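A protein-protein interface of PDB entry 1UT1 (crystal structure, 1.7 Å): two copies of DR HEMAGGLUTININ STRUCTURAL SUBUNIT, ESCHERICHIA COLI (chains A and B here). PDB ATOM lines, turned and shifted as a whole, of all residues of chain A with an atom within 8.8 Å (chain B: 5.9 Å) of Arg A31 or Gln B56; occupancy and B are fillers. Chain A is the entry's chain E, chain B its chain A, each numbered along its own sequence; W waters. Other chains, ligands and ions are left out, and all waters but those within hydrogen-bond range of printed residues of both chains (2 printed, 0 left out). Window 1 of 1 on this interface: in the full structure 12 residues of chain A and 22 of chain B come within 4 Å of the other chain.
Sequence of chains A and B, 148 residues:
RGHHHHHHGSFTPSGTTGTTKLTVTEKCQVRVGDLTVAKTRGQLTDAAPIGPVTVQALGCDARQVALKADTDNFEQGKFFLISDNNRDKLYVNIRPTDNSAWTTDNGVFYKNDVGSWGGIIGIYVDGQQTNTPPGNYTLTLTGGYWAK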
ATOM      1  N   THR A  23      20.756  17.750   0.177  1.00  0.00           N
ATOM      2  CA  THR A  23      20.582  17.022  -1.056  1.00  0.00           C
ATOM      3  C   THR A  23      19.229  17.451  -1.621  1.00  0.00           C
ATOM      4  O   THR A  23      18.199  17.412  -0.927  1.00  0.00           O
ATOM      5  CB  THR A  23      20.651  15.486  -0.857  1.00  0.00           C
ATOM      6  OG1 THR A  23      21.980  15.119  -0.453  1.00  0.00           O
ATOM      7  CG2 THR A  23      20.282  14.731  -2.180  1.00  0.00           C
ATOM      8  N   THR A  25      16.361  16.847  -4.448  1.00  0.00           N
ATOM      9  CA  THR A  25      15.830  15.756  -5.263  1.00  0.00           C
ATOM     10  C   THR A  25      14.656  16.211  -6.157  1.00  0.00           C
ATOM     11  O   THR A  25      14.184  17.358  -6.079  1.00  0.00           O
ATOM     12  CB  THR A  25      15.321  14.580  -4.366  1.00  0.00           C
ATOM     13  OG1 THR A  25      14.042  14.905  -3.800  1.00  0.00           O
ATOM     14  CG2 THR A  25      16.333  14.276  -3.221  1.00  0.00           C
ATOM     15  N   CYS A  28       9.887  12.375  -6.972  1.00  0.00           N
ATOM     16  CA  CYS A  28      10.138  10.950  -6.687  1.00  0.00           C
ATOM     17  C   CYS A  28      11.552  10.927  -6.161  1.00  0.00           C
ATOM     18  O   CYS A  28      12.510  11.227  -6.891  1.00  0.00           O
ATOM     19  CB  CYS A  28      10.027  10.101  -7.949  1.00  0.00           C
ATOM     20  SG  CYS A  28      10.845   8.463  -7.824  1.00  0.00           S
ATOM     21  N   GLN A  29      11.648  10.656  -4.865  1.00  0.00           N
ATOM     22  CA  GLN A  29      12.843  10.841  -4.050  1.00  0.00           C
ATOM     23  C   GLN A  29      13.195   9.495  -3.411  1.00  0.00           C
ATOM     24  O   GLN A  29      12.379   8.933  -2.679  1.00  0.00           O
ATOM     25  CB  GLN A  29      12.457  11.827  -2.924  1.00  0.00           C
ATOM     26  CG  GLN A  29      13.601  12.263  -2.003  1.00  0.00           C
ATOM     27  CD  GLN A  29      13.131  13.238  -0.905  1.00  0.00           C
ATOM     28  OE1 GLN A  29      12.540  12.805   0.063  1.00  0.00           O
ATOM     29  NE2 GLN A  29      13.426  14.547  -1.072  1.00  0.00           N
ATOM     30  N   VAL A  30      14.425   9.019  -3.625  1.00  0.00           N
ATOM     31  CA  VAL A  30      14.832   7.705  -3.098  1.00  0.00           C
ATOM     32  C   VAL A  30      15.953   7.874  -2.075  1.00  0.00           C
ATOM     33  O   VAL A  30      17.071   8.197  -2.404  1.00  0.00           O
ATOM     34  CB  VAL A  30      15.308   6.789  -4.223  1.00  0.00           C
ATOM     35  CG1 VAL A  30      15.720   5.382  -3.639  1.00  0.00           C
ATOM     36  CG2 VAL A  30      14.191   6.686  -5.290  1.00  0.00           C
ATOM     37  N   ARG A  31      15.595   7.718  -0.818  1.00  0.00           N
ATOM     38  CA  ARG A  31      16.546   7.859   0.250  1.00  0.00           C
ATOM     39  C   ARG A  31      17.319   6.543   0.393  1.00  0.00           C
ATOM     40  O   ARG A  31      16.733   5.476   0.416  1.00  0.00           O
ATOM     41  CB  ARG A  31      15.813   8.192   1.537  1.00  0.00           C
ATOM     42  CG  ARG A  31      15.827   7.111   2.538  1.00  0.00           C
ATOM     43  CD  ARG A  31      16.070   7.657   3.915  1.00  0.00           C
ATOM     44  NE  ARG A  31      15.599   6.728   4.934  1.00  0.00           N
ATOM     45  CZ  ARG A  31      15.982   5.458   5.008  1.00  0.00           C
ATOM     46  NH1 ARG A  31      16.855   4.968   4.127  1.00  0.00           N
ATOM     47  NH2 ARG A  31      15.499   4.678   5.962  1.00  0.00           N
ATOM     48  N   VAL A  32      18.643   6.636   0.438  1.00  0.00           N
ATOM     49  CA  VAL A  32      19.498   5.443   0.506  1.00  0.00           C
ATOM     50  C   VAL A  32      20.450   5.626   1.678  1.00  0.00           C
ATOM     51  O   VAL A  32      21.195   6.622   1.741  1.00  0.00           O
ATOM     52  CB  VAL A  32      20.368   5.306  -0.765  1.00  0.00           C
ATOM     53  CG1 VAL A  32      21.253   4.030  -0.687  1.00  0.00           C
ATOM     54  CG2 VAL A  32      19.497   5.306  -2.017  1.00  0.00           C
ATOM     55  N   GLY A  33      20.453   4.657   2.582  1.00  0.00           N
ATOM     56  CA  GLY A  33      21.344   4.701   3.750  1.00  0.00           C
ATOM     57  C   GLY A  33      20.788   5.623   4.846  1.00  0.00           C
ATOM     58  O   GLY A  33      19.597   5.873   4.904  1.00  0.00           O
ATOM     59  N   ASP A  34      21.668   6.124   5.716  1.00  0.00           N
ATOM     60  CA  ASP A  34      21.232   6.963   6.843  1.00  0.00           C
ATOM     61  C   ASP A  34      20.510   8.225   6.412  1.00  0.00           C
ATOM     62  O   ASP A  34      20.773   8.770   5.333  1.00  0.00           O
ATOM     63  CB  ASP A  34      22.426   7.335   7.723  1.00  0.00           C
ATOM     64  CG  ASP A  34      22.922   6.157   8.564  1.00  0.00           C
ATOM     65  OD1 ASP A  34      23.454   6.395   9.673  1.00  0.00           O
ATOM     66  OD2 ASP A  34      22.770   4.995   8.117  1.00  0.00           O
ATOM     67  N   LEU A  35      19.602   8.698   7.260  1.00  0.00           N
ATOM     68  CA  LEU A  35      18.880   9.931   7.000  1.00  0.00           C
ATOM     69  C   LEU A  35      19.862  11.094   6.937  1.00  0.00           C
ATOM     70  O   LEU A  35      20.804  11.170   7.746  1.00  0.00           O
ATOM     71  CB  LEU A  35      17.848  10.196   8.101  1.00  0.00           C
ATOM     72  CG  LEU A  35      16.621   9.275   8.067  1.00  0.00           C
ATOM     73  CD1 LEU A  35      15.657   9.639   9.202  1.00  0.00           C
ATOM     74  CD2 LEU A  35      15.938   9.403   6.706  1.00  0.00           C
ATOM     75  N   THR A  36      19.645  11.975   5.963  1.00  0.00           N
ATOM     76  CA  THR A  36      20.428  13.195   5.784  1.00  0.00           C
ATOM     77  C   THR A  36      19.446  14.287   5.367  1.00  0.00           C
ATOM     78  O   THR A  36      18.305  13.995   5.023  1.00  0.00           O
ATOM     79  CB  THR A  36      21.501  13.030   4.676  1.00  0.00           C
ATOM     80  OG1 THR A  36      20.861  12.729   3.429  1.00  0.00           O
ATOM     81  CG2 THR A  36      22.458  11.899   5.015  1.00  0.00           C
ATOM     82  N   ALA A  38      17.491  16.484   3.170  1.00  0.00           N
ATOM     83  CA  ALA A  38      17.150  16.451   1.751  1.00  0.00           C
ATOM     84  C   ALA A  38      15.872  17.224   1.563  1.00  0.00           C
ATOM     85  O   ALA A  38      15.012  17.239   2.468  1.00  0.00           O
ATOM     86  CB  ALA A  38      16.941  15.031   1.303  1.00  0.00           C
ATOM     87  N   SER B  14      17.979  11.127  -8.085  1.00  0.00           N
ATOM     88  CA  SER B  14      16.944  11.825  -7.299  1.00  0.00           C
ATOM     89  C   SER B  14      16.767  11.130  -5.950  1.00  0.00           C
ATOM     90  O   SER B  14      15.930  10.248  -5.795  1.00  0.00           O
ATOM     91  CB  SER B  14      15.592  11.872  -8.053  1.00  0.00           C
ATOM     92  OG  SER B  14      14.670  12.651  -7.302  1.00  0.00           O
ATOM     93  N   GLY B  15      17.609  11.503  -5.005  1.00  0.00           N
ATOM     94  CA  GLY B  15      17.624  10.828  -3.717  1.00  0.00           C
ATOM     95  C   GLY B  15      18.960  11.059  -3.031  1.00  0.00           C
ATOM     96  O   GLY B  15      19.813  11.827  -3.501  1.00  0.00           O
ATOM     97  N   THR B  16      19.204  10.287  -1.998  1.00  0.00           N
ATOM     98  CA  THR B  16      20.452  10.381  -1.304  1.00  0.00           C
ATOM     99  C   THR B  16      21.425   9.213  -1.632  1.00  0.00           C
ATOM    100  O   THR B  16      21.112   8.310  -2.402  1.00  0.00           O
ATOM    101  CB  THR B  16      20.232  10.538   0.167  1.00  0.00           C
ATOM    102  OG1 THR B  16      19.472   9.423   0.658  1.00  0.00           O
ATOM    103  CG2 THR B  16      19.425  11.839   0.406  1.00  0.00           C
ATOM    104  N   THR B  54      19.529   0.516   3.711  1.00  0.00           N
ATOM    105  CA  THR B  54      18.095   0.762   3.785  1.00  0.00           C
ATOM    106  C   THR B  54      17.675   1.704   2.645  1.00  0.00           C
ATOM    107  O   THR B  54      18.429   2.608   2.243  1.00  0.00           O
ATOM    108  CB  THR B  54      17.681   1.356   5.150  1.00  0.00           C
ATOM    109  OG1 THR B  54      18.374   2.589   5.345  1.00  0.00           O
ATOM    110  CG2 THR B  54      18.049   0.392   6.283  1.00  0.00           C
ATOM    111  N   VAL B  55      16.513   1.434   2.071  1.00  0.00           N
ATOM    112  CA  VAL B  55      16.031   2.267   0.963  1.00  0.00           C
ATOM    113  C   VAL B  55      14.601   2.664   1.250  1.00  0.00           C
ATOM    114  O   VAL B  55      13.778   1.837   1.649  1.00  0.00           O
ATOM    115  CB  VAL B  55      16.061   1.505  -0.385  1.00  0.00           C
ATOM    116  CG1 VAL B  55      15.381   2.347  -1.527  1.00  0.00           C
ATOM    117  CG2 VAL B  55      17.491   1.125  -0.757  1.00  0.00           C
ATOM    118  N   GLN B  56      14.286   3.933   1.048  1.00  0.00           N
ATOM    119  CA  GLN B  56      12.885   4.346   1.150  1.00  0.00           C
ATOM    120  C   GLN B  56      12.553   5.377   0.127  1.00  0.00           C
ATOM    121  O   GLN B  56      13.122   6.480   0.138  1.00  0.00           O
ATOM    122  CB  GLN B  56      12.505   4.852   2.526  1.00  0.00           C
ATOM    123  CG  GLN B  56      11.036   5.291   2.584  1.00  0.00           C
ATOM    124  CD  GLN B  56      10.092   4.107   2.474  1.00  0.00           C
ATOM    125  OE1 GLN B  56      10.137   3.196   3.309  1.00  0.00           O
ATOM    126  NE2 GLN B  56       9.362   4.029   1.372  1.00  0.00           N
ATOM    127  N   ALA B  57      11.652   5.017  -0.779  1.00  0.00           N
ATOM    128  CA  ALA B  57      11.264   5.921  -1.871  1.00  0.00           C
ATOM    129  C   ALA B  57       9.948   6.582  -1.494  1.00  0.00           C
ATOM    130  O   ALA B  57       9.099   5.967  -0.856  1.00  0.00           O
ATOM    131  CB  ALA B  57      11.111   5.137  -3.215  1.00  0.00           C
ATOM    132  N   LEU B  58       9.798   7.841  -1.880  1.00  0.00           N
ATOM    133  CA  LEU B  58       8.547   8.582  -1.679  1.00  0.00           C
ATOM    134  C   LEU B  58       8.259   9.330  -2.975  1.00  0.00           C
ATOM    135  O   LEU B  58       9.177   9.864  -3.581  1.00  0.00           O
ATOM    136  CB  LEU B  58       8.692   9.598  -0.529  1.00  0.00           C
ATOM    137  CG  LEU B  58       9.087   9.028   0.853  1.00  0.00           C
ATOM    138  CD1 LEU B  58      10.576   9.351   1.197  1.00  0.00           C
ATOM    139  CD2 LEU B  58       8.151   9.537   1.955  1.00  0.00           C
ATOM    140  N   SER B 116       6.518   3.329  -4.919  1.00  0.00           N
ATOM    141  CA  SER B 116       7.385   3.911  -3.900  1.00  0.00           C
ATOM    142  C   SER B 116       7.870   2.829  -2.938  1.00  0.00           C
ATOM    143  O   SER B 116       7.407   2.737  -1.815  1.00  0.00           O
ATOM    144  CB  SER B 116       6.613   4.986  -3.131  1.00  0.00           C
ATOM    145  OG  SER B 116       6.345   6.074  -3.997  1.00  0.00           O
ATOM    146  N   TRP B 117       8.821   2.025  -3.393  1.00  0.00           N
ATOM    147  CA  TRP B 117       9.329   0.910  -2.610  1.00  0.00           C
ATOM    148  C   TRP B 117      10.137   1.381  -1.399  1.00  0.00           C
ATOM    149  O   TRP B 117      10.934   2.337  -1.491  1.00  0.00           O
ATOM    150  CB  TRP B 117      10.237   0.054  -3.497  1.00  0.00           C
ATOM    151  CG  TRP B 117      10.693  -1.189  -2.854  1.00  0.00           C
ATOM    152  CD1 TRP B 117       9.954  -2.335  -2.665  1.00  0.00           C
ATOM    153  CD2 TRP B 117      12.018  -1.474  -2.358  1.00  0.00           C
ATOM    154  NE1 TRP B 117      10.747  -3.313  -2.107  1.00  0.00           N
ATOM    155  CE2 TRP B 117      12.008  -2.812  -1.895  1.00  0.00           C
ATOM    156  CE3 TRP B 117      13.210  -0.724  -2.256  1.00  0.00           C
ATOM    157  CZ2 TRP B 117      13.145  -3.433  -1.354  1.00  0.00           C
ATOM    158  CZ3 TRP B 117      14.345  -1.347  -1.707  1.00  0.00           C
ATOM    159  CH2 TRP B 117      14.293  -2.688  -1.248  1.00  0.00           C
ATOM    160  N   GLY B 118      10.030   0.609  -0.320  1.00  0.00           N
ATOM    161  CA  GLY B 118      10.879   0.771   0.842  1.00  0.00           C
ATOM    162  C   GLY B 118      11.313  -0.648   1.195  1.00  0.00           C
ATOM    163  O   GLY B 118      10.541  -1.612   1.035  1.00  0.00           O
ATOM    164  N   GLY B 119      12.535  -0.784   1.665  1.00  0.00           N
ATOM    165  CA  GLY B 119      13.047  -2.101   1.994  1.00  0.00           C
ATOM    166  C   GLY B 119      14.528  -2.073   2.377  1.00  0.00           C
ATOM    167  O   GLY B 119      15.108  -1.033   2.680  1.00  0.00           O
ATOM    168  N   GLY B 143      20.362   7.004  -4.896  1.00  0.00           N
ATOM    169  CA  GLY B 143      18.963   6.758  -5.221  1.00  0.00           C
ATOM    170  C   GLY B 143      18.486   7.608  -6.363  1.00  0.00           C
ATOM    171  O   GLY B 143      18.977   8.728  -6.592  1.00  0.00           O
HETATM  172  O   HOH W   1      20.548   3.482   7.456  1.00  0.00           O
HETATM  173  O   HOH W   2      19.184   9.676   3.155  1.00  0.00           O
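No position is printed for both chains.
Water W2 lies within hydrogen-bond range of OG1 of Thr B16 (2.5 Å), O of Asp A34 (2.8 Å) and OG1 of Thr A36 (3.5 Å). Water W1 bridges the side-chain carboxylate (OD2) of Asp A34 and the side-chain hydroxyl (OG1) of Thr B54.
The backbone carbonyl oxygen of Thr B16 is in hydrogen-bond range of the backbone NH of Gly B143. O of Val B55 lies within hydrogen-bond range of N of Gly B119 (2.9 Å). The guanidinium group (NH1) of Arg A31 sits at hydrogen-bond distance from the backbone carbonyl oxygen (O) of Gly A33 (3.0 Å). OG1 of Thr A25 is in hydrogen-bond range of NE2 of Gln A29. N of Ser B14 lies within hydrogen-bond range of O of Gly B143, at 3.0 Å. The backbone NH (N) of Ala B57 sits at hydrogen-bond distance from the backbone carbonyl oxygen (O) of Trp B117, 2.9 Å away.
Among the printed residues, merely in contact across the chains: Thr A23 with Gly B15, Thr A23 with Thr B16, Thr A25 with Ser B14, Thr A25 with Gly B15, Cys A28 with Leu B58, Gln A29 with Ser B14, Gln A29 with Gln B56, Gln A29 with Ala B57, Val A30 with Gly B15, Val A30 with Val B55, Val A30 with Gln B56, Val A30 with Gly B143, Arg A31 with Thr B16, Arg A31 with Val B55, Val A32 with Thr B54, Val A32 with Gly B143 and Thr A36 with Thr B16.
Of the 13 printed residues of chain B, 9 touch a printed residue of chain A. Along chain B the printed residues that touch a printed residue of chain A span positions 14 to 143. Printed residues of chain A that touch a printed residue of chain B: Thr A23, Thr A25, Cys A28, Gln A29, Val A30, Arg A31, Val A32, Gly A33 and Thr A36. Hydrophobic or aromatic side chains of chain A that line the printed part of chain B: Val A30 and Val A32. Among the printed residues, no Asp or Glu carboxylate lies within 4 Å of a Lys or Arg side-chain nitrogen of the other chain.
The side-chain hydroxyl (OG1) of Thr B16 lies within hydrogen-bond range of the backbone NH (N) of Val A32 (2.9 Å). The side-chain hydroxyl (OG) of Ser B14 sits at hydrogen-bond distance from the backbone carbonyl oxygen (O) of Cys A28 (2.6 Å). The backbone carbonyl oxygen (O) of Ser B14 sits at hydrogen-bond distance from the backbone NH (N) of Val A30. The backbone NH of Arg A31 lies within hydrogen-bond range of the backbone carbonyl oxygen of Gln B56 (2.9 Å). The side-chain hydroxyl of Thr B54 lies within hydrogen-bond range of the guanidinium group of Arg A31 (3.1 Å). O of Thr B54 sits at hydrogen-bond distance from N of Gly A33 (2.9 Å). O of Val A30 is in hydrogen-bond range of N of Thr B16, at 3.0 Å. N of Gln A29 sits at hydrogen-bond distance from O of Leu B58, at 2.9 Å.
Printed residues of chain B within 4 Å of Arg A31: Thr B16 (3.3 Å), Thr B54 (3.1 Å), Val B55 (3.3 Å) and Gln B56 (2.9 Å). Of the printed residues of chain A, Gln B56 touches Gln A29, Val A30 and Arg A31. Of the printed residues of chain A, Gly B143 touches Val A30 (3.7 Å) and Val A32 (3.5 Å). Of the printed residues of chain B, Val A32 touches Thr B16, Thr B54 and Gly B143. Of the printed residues of chain A, Thr B16 touches Thr A23, Val A30, Arg A31, Val A32 and Thr A36. The nearest printed residue of chain A that does not touch Gln B56 is Val A32 (5.2 Å). The nearest printed residue of chain A that does not touch Ser B14 is Arg A31 (5.6 Å).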
